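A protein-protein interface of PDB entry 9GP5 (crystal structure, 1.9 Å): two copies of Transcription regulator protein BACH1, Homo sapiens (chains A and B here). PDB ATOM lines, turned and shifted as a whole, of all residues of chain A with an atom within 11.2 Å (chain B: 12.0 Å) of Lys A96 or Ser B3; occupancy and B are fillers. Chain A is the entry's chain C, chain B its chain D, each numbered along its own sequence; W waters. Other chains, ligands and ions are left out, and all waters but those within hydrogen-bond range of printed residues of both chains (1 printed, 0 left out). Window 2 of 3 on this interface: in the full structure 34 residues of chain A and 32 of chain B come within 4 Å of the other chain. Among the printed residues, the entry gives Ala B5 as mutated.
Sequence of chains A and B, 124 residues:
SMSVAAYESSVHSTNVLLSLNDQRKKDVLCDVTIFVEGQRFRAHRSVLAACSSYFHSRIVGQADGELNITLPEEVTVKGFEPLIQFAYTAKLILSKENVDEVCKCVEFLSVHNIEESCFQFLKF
Printed residues of chain B that touch a printed residue of chain A: Ser B3, Val B4, Ala B5, Ala B6 and Tyr B7. Hydrophobic or aromatic side chains of chain B that line the printed part of chain A: Val B4 and Tyr B7. Along chain B the printed residues that touch a printed residue of chain A span positions 3 to 7. Hydrophobic or aromatic side chains of chain A that line the printed part of chain B: Ile A93 and Leu A94. Among the printed residues, 9 pairs touch across the chains.
O of Leu A92 is in hydrogen-bond range of N of Tyr B7 (2.8 Å). N of Ala B5 is in hydrogen-bond range of O of Leu A94 (2.9 Å). The backbone NH (N) of Lys A96 sits at hydrogen-bond distance from the backbone carbonyl oxygen (O) of Ser B3 (3.0 Å).
No position is printed for both chains. Of the 9 pairs that touch across the chains among the printed residues, none has its exchanged pair printed and touching as well.
Ala B5 touches Leu A92 (O to O, 3.6 Å). O of Leu A92 touches CA of Ala B6, 3.5 Å away. Ile A93 touches Ala B5. O of Leu A94 touches CA of Val B4, 3.4 Å away. CD1 of Leu A94 touches CE2 of Tyr B7, 3.97 Å away. Ser A95 touches Ser B3.
Water W1 lies within hydrogen-bond range of OE1 of Glu A97 (2.7 Å) and O of Ser B3 (2.8 Å).
The backbone NH (N) of Glu A97 lies close to the side-chain hydroxyl (OG) of Ser A95, at 3.2 Å. The backbone NH (N) of Ser A95 sits at hydrogen-bond distance from the side-chain amide oxygen (OD1) of Asn A98 (2.8 Å).
Printed residues of chain B within 4 Å of Leu A92: Ala B5 (3.6 Å), Ala B6 (3.5 Å) and Tyr B7 (2.8 Å). Printed residues of chain B within 4 Å of Ile A93: Ala B5 (3.4 Å). Leu A94 touches three residues of chain B. Of chain B, only Ser B3 (3.0 Å) comes within 4 Å of Lys A96. No residue of chain B comes within 4 Å of Glu A97. Asn A98 touches none of the printed residues of chain B. No residue of chain B comes within 4 Å of Val A99. Glu A101 touches none of the printed residues of chain B. Cys A103 touches none of the printed residues of chain B. Ser B3 touches two residues of chain A. Val B4 touches one residue of chain A. Of the printed residues of chain A, Ala B5 touches Leu A92, Ile A93 and Leu A94. Of the printed residues of chain A, Ala B6 touches Leu A92. Printed residues of chain A within 4 Å of Tyr B7: Leu A92 (2.8 Å) and Leu A94 (3.97 Å). The nearest residue of chain B that does not touch Lys A96 is Met B2 (4.4 Å). The nearest residue of chain A that does not touch Ser B3 is Leu A94 (4.3 Å). The nearest printed residue of chain B that does not touch Ile A93 is Ala B6 (4.5 Å).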
ATOM      1  N   LYS A  78      35.356 -26.542 -20.181  1.00  0.00           N
ATOM      2  CA  LYS A  78      33.997 -26.473 -20.691  1.00  0.00           C
ATOM      3  C   LYS A  78      33.858 -25.409 -21.784  1.00  0.00           C
ATOM      4  O   LYS A  78      33.039 -25.546 -22.679  1.00  0.00           O
ATOM      5  CB  LYS A  78      33.015 -26.136 -19.569  1.00  0.00           C
ATOM      6  CG  LYS A  78      32.006 -27.212 -19.226  1.00  0.00           C
ATOM      7  CD  LYS A  78      30.832 -26.655 -18.427  1.00  0.00           C
ATOM      8  CE  LYS A  78      29.939 -27.759 -17.903  1.00  0.00           C
ATOM      9  NZ  LYS A  78      30.639 -28.628 -16.918  1.00  0.00           N
ATOM     10  N   GLY A  79      34.576 -24.295 -21.654  1.00  0.00           N
ATOM     11  CA  GLY A  79      34.466 -23.210 -22.613  1.00  0.00           C
ATOM     12  C   GLY A  79      35.441 -23.365 -23.765  1.00  0.00           C
ATOM     13  O   GLY A  79      35.201 -22.859 -24.848  1.00  0.00           O
ATOM     14  N   PRO A  82      34.700 -26.685 -26.964  1.00  0.00           N
ATOM     15  CA  PRO A  82      33.889 -26.393 -28.143  1.00  0.00           C
ATOM     16  C   PRO A  82      34.592 -25.483 -29.165  1.00  0.00           C
ATOM     17  O   PRO A  82      34.360 -25.600 -30.384  1.00  0.00           O
ATOM     18  CB  PRO A  82      32.652 -25.707 -27.604  1.00  0.00           C
ATOM     19  CG  PRO A  82      32.619 -26.095 -26.149  1.00  0.00           C
ATOM     20  CD  PRO A  82      34.080 -26.181 -25.746  1.00  0.00           C
ATOM     21  N   LEU A  92      30.413 -25.496 -34.521  1.00  0.00           N
ATOM     22  CA  LEU A  92      30.337 -25.054 -33.137  1.00  0.00           C
ATOM     23  C   LEU A  92      29.020 -25.520 -32.515  1.00  0.00           C
ATOM     24  O   LEU A  92      27.939 -25.186 -33.018  1.00  0.00           O
ATOM     25  CB  LEU A  92      30.473 -23.529 -33.076  1.00  0.00           C
ATOM     26  CG  LEU A  92      30.414 -22.930 -31.658  1.00  0.00           C
ATOM     27  CD1 LEU A  92      31.553 -23.413 -30.785  1.00  0.00           C
ATOM     28  CD2 LEU A  92      30.416 -21.414 -31.711  1.00  0.00           C
ATOM     29  N   ILE A  93      29.118 -26.236 -31.383  1.00  0.00           N
ATOM     30  CA  ILE A  93      27.924 -26.636 -30.667  1.00  0.00           C
ATOM     31  C   ILE A  93      27.932 -25.932 -29.333  1.00  0.00           C
ATOM     32  O   ILE A  93      28.916 -26.076 -28.597  1.00  0.00           O
ATOM     33  CB  ILE A  93      27.863 -28.157 -30.445  1.00  0.00           C
ATOM     34  CG1 ILE A  93      28.059 -28.956 -31.729  1.00  0.00           C
ATOM     35  CG2 ILE A  93      26.577 -28.487 -29.722  1.00  0.00           C
ATOM     36  CD1 ILE A  93      27.877 -30.430 -31.536  1.00  0.00           C
ATOM     37  N   LEU A  94      26.823 -25.233 -29.074  1.00  0.00           N
ATOM     38  CA  LEU A  94      26.538 -24.534 -27.844  1.00  0.00           C
ATOM     39  C   LEU A  94      25.310 -25.157 -27.172  1.00  0.00           C
ATOM     40  O   LEU A  94      24.350 -25.572 -27.817  1.00  0.00           O
ATOM     41  CB  LEU A  94      26.264 -23.064 -28.169  1.00  0.00           C
ATOM     42  CG  LEU A  94      27.417 -22.281 -28.815  1.00  0.00           C
ATOM     43  CD1 LEU A  94      27.020 -20.816 -28.897  1.00  0.00           C
ATOM     44  CD2 LEU A  94      28.688 -22.456 -28.014  1.00  0.00           C
ATOM     45  N   SER A  95      25.363 -25.220 -25.858  1.00  0.00           N
ATOM     46  CA  SER A  95      24.222 -25.632 -25.063  1.00  0.00           C
ATOM     47  C   SER A  95      23.936 -24.552 -24.038  1.00  0.00           C
ATOM     48  O   SER A  95      24.810 -23.764 -23.708  1.00  0.00           O
ATOM     49  CB  SER A  95      24.538 -26.916 -24.385  1.00  0.00           C
ATOM     50  OG  SER A  95      25.580 -26.730 -23.411  1.00  0.00           O
ATOM     51  N   LYS A  96      22.776 -24.618 -23.411  1.00  0.00           N
ATOM     52  CA  LYS A  96      22.474 -23.652 -22.376  1.00  0.00           C
ATOM     53  C   LYS A  96      23.494 -23.890 -21.255  1.00  0.00           C
ATOM     54  O   LYS A  96      23.816 -22.974 -20.538  1.00  0.00           O
ATOM     55  CB  LYS A  96      20.993 -23.710 -21.983  1.00  0.00           C
ATOM     56  CG  LYS A  96      20.670 -24.470 -20.705  1.00  0.00           C
ATOM     57  CD  LYS A  96      19.254 -24.315 -20.171  1.00  0.00           C
ATOM     58  CE  LYS A  96      18.153 -24.661 -21.160  1.00  0.00           C
ATOM     59  NZ  LYS A  96      18.180 -26.083 -21.595  1.00  0.00           N
ATOM     60  N   GLU A  97      24.058 -25.102 -21.146  1.00  0.00           N
ATOM     61  CA  GLU A  97      24.949 -25.440 -20.047  1.00  0.00           C
ATOM     62  C   GLU A  97      26.335 -24.817 -20.255  1.00  0.00           C
ATOM     63  O   GLU A  97      26.997 -24.458 -19.281  1.00  0.00           O
ATOM     64  CB  GLU A  97      25.056 -26.963 -19.906  1.00  0.00           C
ATOM     65  CG  GLU A  97      23.788 -27.589 -19.292  1.00  0.00           C
ATOM     66  CD  GLU A  97      22.568 -27.759 -20.196  1.00  0.00           C
ATOM     67  OE1 GLU A  97      22.721 -27.724 -21.435  1.00  0.00           O
ATOM     68  OE2 GLU A  97      21.436 -27.933 -19.640  1.00  0.00           O
ATOM     69  N   ASN A  98      26.763 -24.665 -21.509  1.00  0.00           N
ATOM     70  CA  ASN A  98      28.140 -24.255 -21.770  1.00  0.00           C
ATOM     71  C   ASN A  98      28.259 -22.859 -22.387  1.00  0.00           C
ATOM     72  O   ASN A  98      29.381 -22.350 -22.537  1.00  0.00           O
ATOM     73  CB  ASN A  98      28.873 -25.283 -22.623  1.00  0.00           C
ATOM     74  CG  ASN A  98      28.524 -25.264 -24.098  1.00  0.00           C
ATOM     75  OD1 ASN A  98      27.773 -24.412 -24.585  1.00  0.00           O
ATOM     76  ND2 ASN A  98      29.106 -26.201 -24.824  1.00  0.00           N
ATOM     77  N   VAL A  99      27.134 -22.223 -22.724  1.00  0.00           N
ATOM     78  CA  VAL A  99      27.143 -20.991 -23.504  1.00  0.00           C
ATOM     79  C   VAL A  99      27.903 -19.869 -22.763  1.00  0.00           C
ATOM     80  O   VAL A  99      28.737 -19.199 -23.376  1.00  0.00           O
ATOM     81  CB  VAL A  99      25.722 -20.577 -23.950  1.00  0.00           C
ATOM     82  CG1 VAL A  99      24.786 -20.198 -22.814  1.00  0.00           C
ATOM     83  CG2 VAL A  99      25.754 -19.471 -24.986  1.00  0.00           C
ATOM     84  N   ASP A 100      27.724 -19.712 -21.454  1.00  0.00           N
ATOM     85  CA  ASP A 100      28.386 -18.615 -20.745  1.00  0.00           C
ATOM     86  C   ASP A 100      29.911 -18.754 -20.778  1.00  0.00           C
ATOM     87  O   ASP A 100      30.611 -17.766 -20.989  1.00  0.00           O
ATOM     88  CB  ASP A 100      27.868 -18.488 -19.314  1.00  0.00           C
ATOM     89  CG  ASP A 100      26.441 -17.957 -19.227  1.00  0.00           C
ATOM     90  OD1 ASP A 100      25.919 -17.513 -20.251  1.00  0.00           O
ATOM     91  OD2 ASP A 100      25.860 -17.976 -18.119  1.00  0.00           O
ATOM     92  N   GLU A 101      30.422 -19.985 -20.623  1.00  0.00           N
ATOM     93  CA  GLU A 101      31.847 -20.230 -20.609  1.00  0.00           C
ATOM     94  C   GLU A 101      32.438 -20.115 -22.003  1.00  0.00           C
ATOM     95  O   GLU A 101      33.583 -19.671 -22.151  1.00  0.00           O
ATOM     96  CB  GLU A 101      32.162 -21.558 -19.930  1.00  0.00           C
ATOM     97  CG  GLU A 101      32.265 -21.323 -18.437  1.00  0.00           C
ATOM     98  CD  GLU A 101      32.202 -22.536 -17.551  1.00  0.00           C
ATOM     99  OE1 GLU A 101      32.942 -23.503 -17.814  1.00  0.00           O
ATOM    100  OE2 GLU A 101      31.449 -22.467 -16.564  1.00  0.00           O
ATOM    101  N   VAL A 102      31.703 -20.583 -23.019  1.00  0.00           N
ATOM    102  CA  VAL A 102      32.224 -20.461 -24.359  1.00  0.00           C
ATOM    103  C   VAL A 102      32.317 -18.980 -24.699  1.00  0.00           C
ATOM    104  O   VAL A 102      33.319 -18.581 -25.291  1.00  0.00           O
ATOM    105  CB  VAL A 102      31.398 -21.268 -25.368  1.00  0.00           C
ATOM    106  CG1 VAL A 102      31.847 -20.978 -26.786  1.00  0.00           C
ATOM    107  CG2 VAL A 102      31.536 -22.763 -25.100  1.00  0.00           C
ATOM    108  N   CYS A 103      31.284 -18.201 -24.374  1.00  0.00           N
ATOM    109  CA  CYS A 103      31.315 -16.769 -24.621  1.00  0.00           C
ATOM    110  C   CYS A 103      32.557 -16.137 -23.991  1.00  0.00           C
ATOM    111  O   CYS A 103      33.258 -15.364 -24.637  1.00  0.00           O
ATOM    112  CB  CYS A 103      30.139 -16.030 -24.014  1.00  0.00           C
ATOM    113  SG  CYS A 103      28.670 -16.177 -25.038  1.00  0.00           S
ATOM    114  N   MET B   2      16.574 -21.127 -26.605  1.00  0.00           N
ATOM    115  CA  MET B   2      17.013 -22.414 -27.219  1.00  0.00           C
ATOM    116  C   MET B   2      17.931 -23.145 -26.240  1.00  0.00           C
ATOM    117  O   MET B   2      18.663 -22.528 -25.483  1.00  0.00           O
ATOM    118  CB  MET B   2      17.737 -22.183 -28.545  1.00  0.00           C
ATOM    119  CG  MET B   2      16.864 -21.498 -29.575  1.00  0.00           C
ATOM    120  SD  MET B   2      15.367 -22.451 -30.006  1.00  0.00           S
ATOM    121  CE  MET B   2      14.714 -21.494 -31.379  1.00  0.00           C
ATOM    122  N   SER B   3      17.854 -24.476 -26.259  1.00  0.00           N
ATOM    123  CA  SER B   3      18.600 -25.344 -25.366  1.00  0.00           C
ATOM    124  C   SER B   3      19.931 -25.777 -25.994  1.00  0.00           C
ATOM    125  O   SER B   3      20.900 -26.052 -25.296  1.00  0.00           O
ATOM    126  CB  SER B   3      17.705 -26.510 -25.033  1.00  0.00           C
ATOM    127  OG  SER B   3      18.448 -27.592 -24.496  1.00  0.00           O
ATOM    128  N   VAL B   4      19.950 -25.889 -27.325  1.00  0.00           N
ATOM    129  CA  VAL B   4      21.069 -26.391 -28.093  1.00  0.00           C
ATOM    130  C   VAL B   4      21.109 -25.591 -29.392  1.00  0.00           C
ATOM    131  O   VAL B   4      20.053 -25.276 -29.943  1.00  0.00           O
ATOM    132  CB  VAL B   4      20.932 -27.893 -28.425  1.00  0.00           C
ATOM    133  CG1 VAL B   4      22.066 -28.353 -29.315  1.00  0.00           C
ATOM    134  CG2 VAL B   4      20.882 -28.756 -27.180  1.00  0.00           C
ATOM    135  N   ALA B   5      22.314 -25.237 -29.813  1.00  0.00           N
ATOM    136  CA  ALA B   5      22.529 -24.616 -31.116  1.00  0.00           C
ATOM    137  C   ALA B   5      23.737 -25.249 -31.783  1.00  0.00           C
ATOM    138  O   ALA B   5      24.819 -25.295 -31.181  1.00  0.00           O
ATOM    139  CB  ALA B   5      22.697 -23.144 -30.926  1.00  0.00           C
ATOM    140  N   ALA B   6      23.568 -25.764 -33.003  1.00  0.00           N
ATOM    141  CA  ALA B   6      24.663 -26.328 -33.762  1.00  0.00           C
ATOM    142  C   ALA B   6      24.915 -25.474 -35.003  1.00  0.00           C
ATOM    143  O   ALA B   6      24.039 -25.366 -35.862  1.00  0.00           O
ATOM    144  CB  ALA B   6      24.343 -27.745 -34.135  1.00  0.00           C
ATOM    145  N   TYR B   7      26.096 -24.865 -35.044  1.00  0.00           N
ATOM    146  CA  TYR B   7      26.476 -23.934 -36.091  1.00  0.00           C
ATOM    147  C   TYR B   7      27.510 -24.569 -36.988  1.00  0.00           C
ATOM    148  O   TYR B   7      28.358 -25.347 -36.514  1.00  0.00           O
ATOM    149  CB  TYR B   7      27.086 -22.666 -35.483  1.00  0.00           C
ATOM    150  CG  TYR B   7      26.121 -21.860 -34.663  1.00  0.00           C
ATOM    151  CD1 TYR B   7      25.144 -21.042 -35.210  1.00  0.00           C
ATOM    152  CD2 TYR B   7      26.193 -21.937 -33.290  1.00  0.00           C
ATOM    153  CE1 TYR B   7      24.288 -20.290 -34.402  1.00  0.00           C
ATOM    154  CE2 TYR B   7      25.371 -21.192 -32.484  1.00  0.00           C
ATOM    155  CZ  TYR B   7      24.423 -20.359 -33.026  1.00  0.00           C
ATOM    156  OH  TYR B   7      23.688 -19.740 -32.024  1.00  0.00           O
HETATM  157  O   HOH W   1      21.108 -28.220 -23.507  1.00  0.00           O
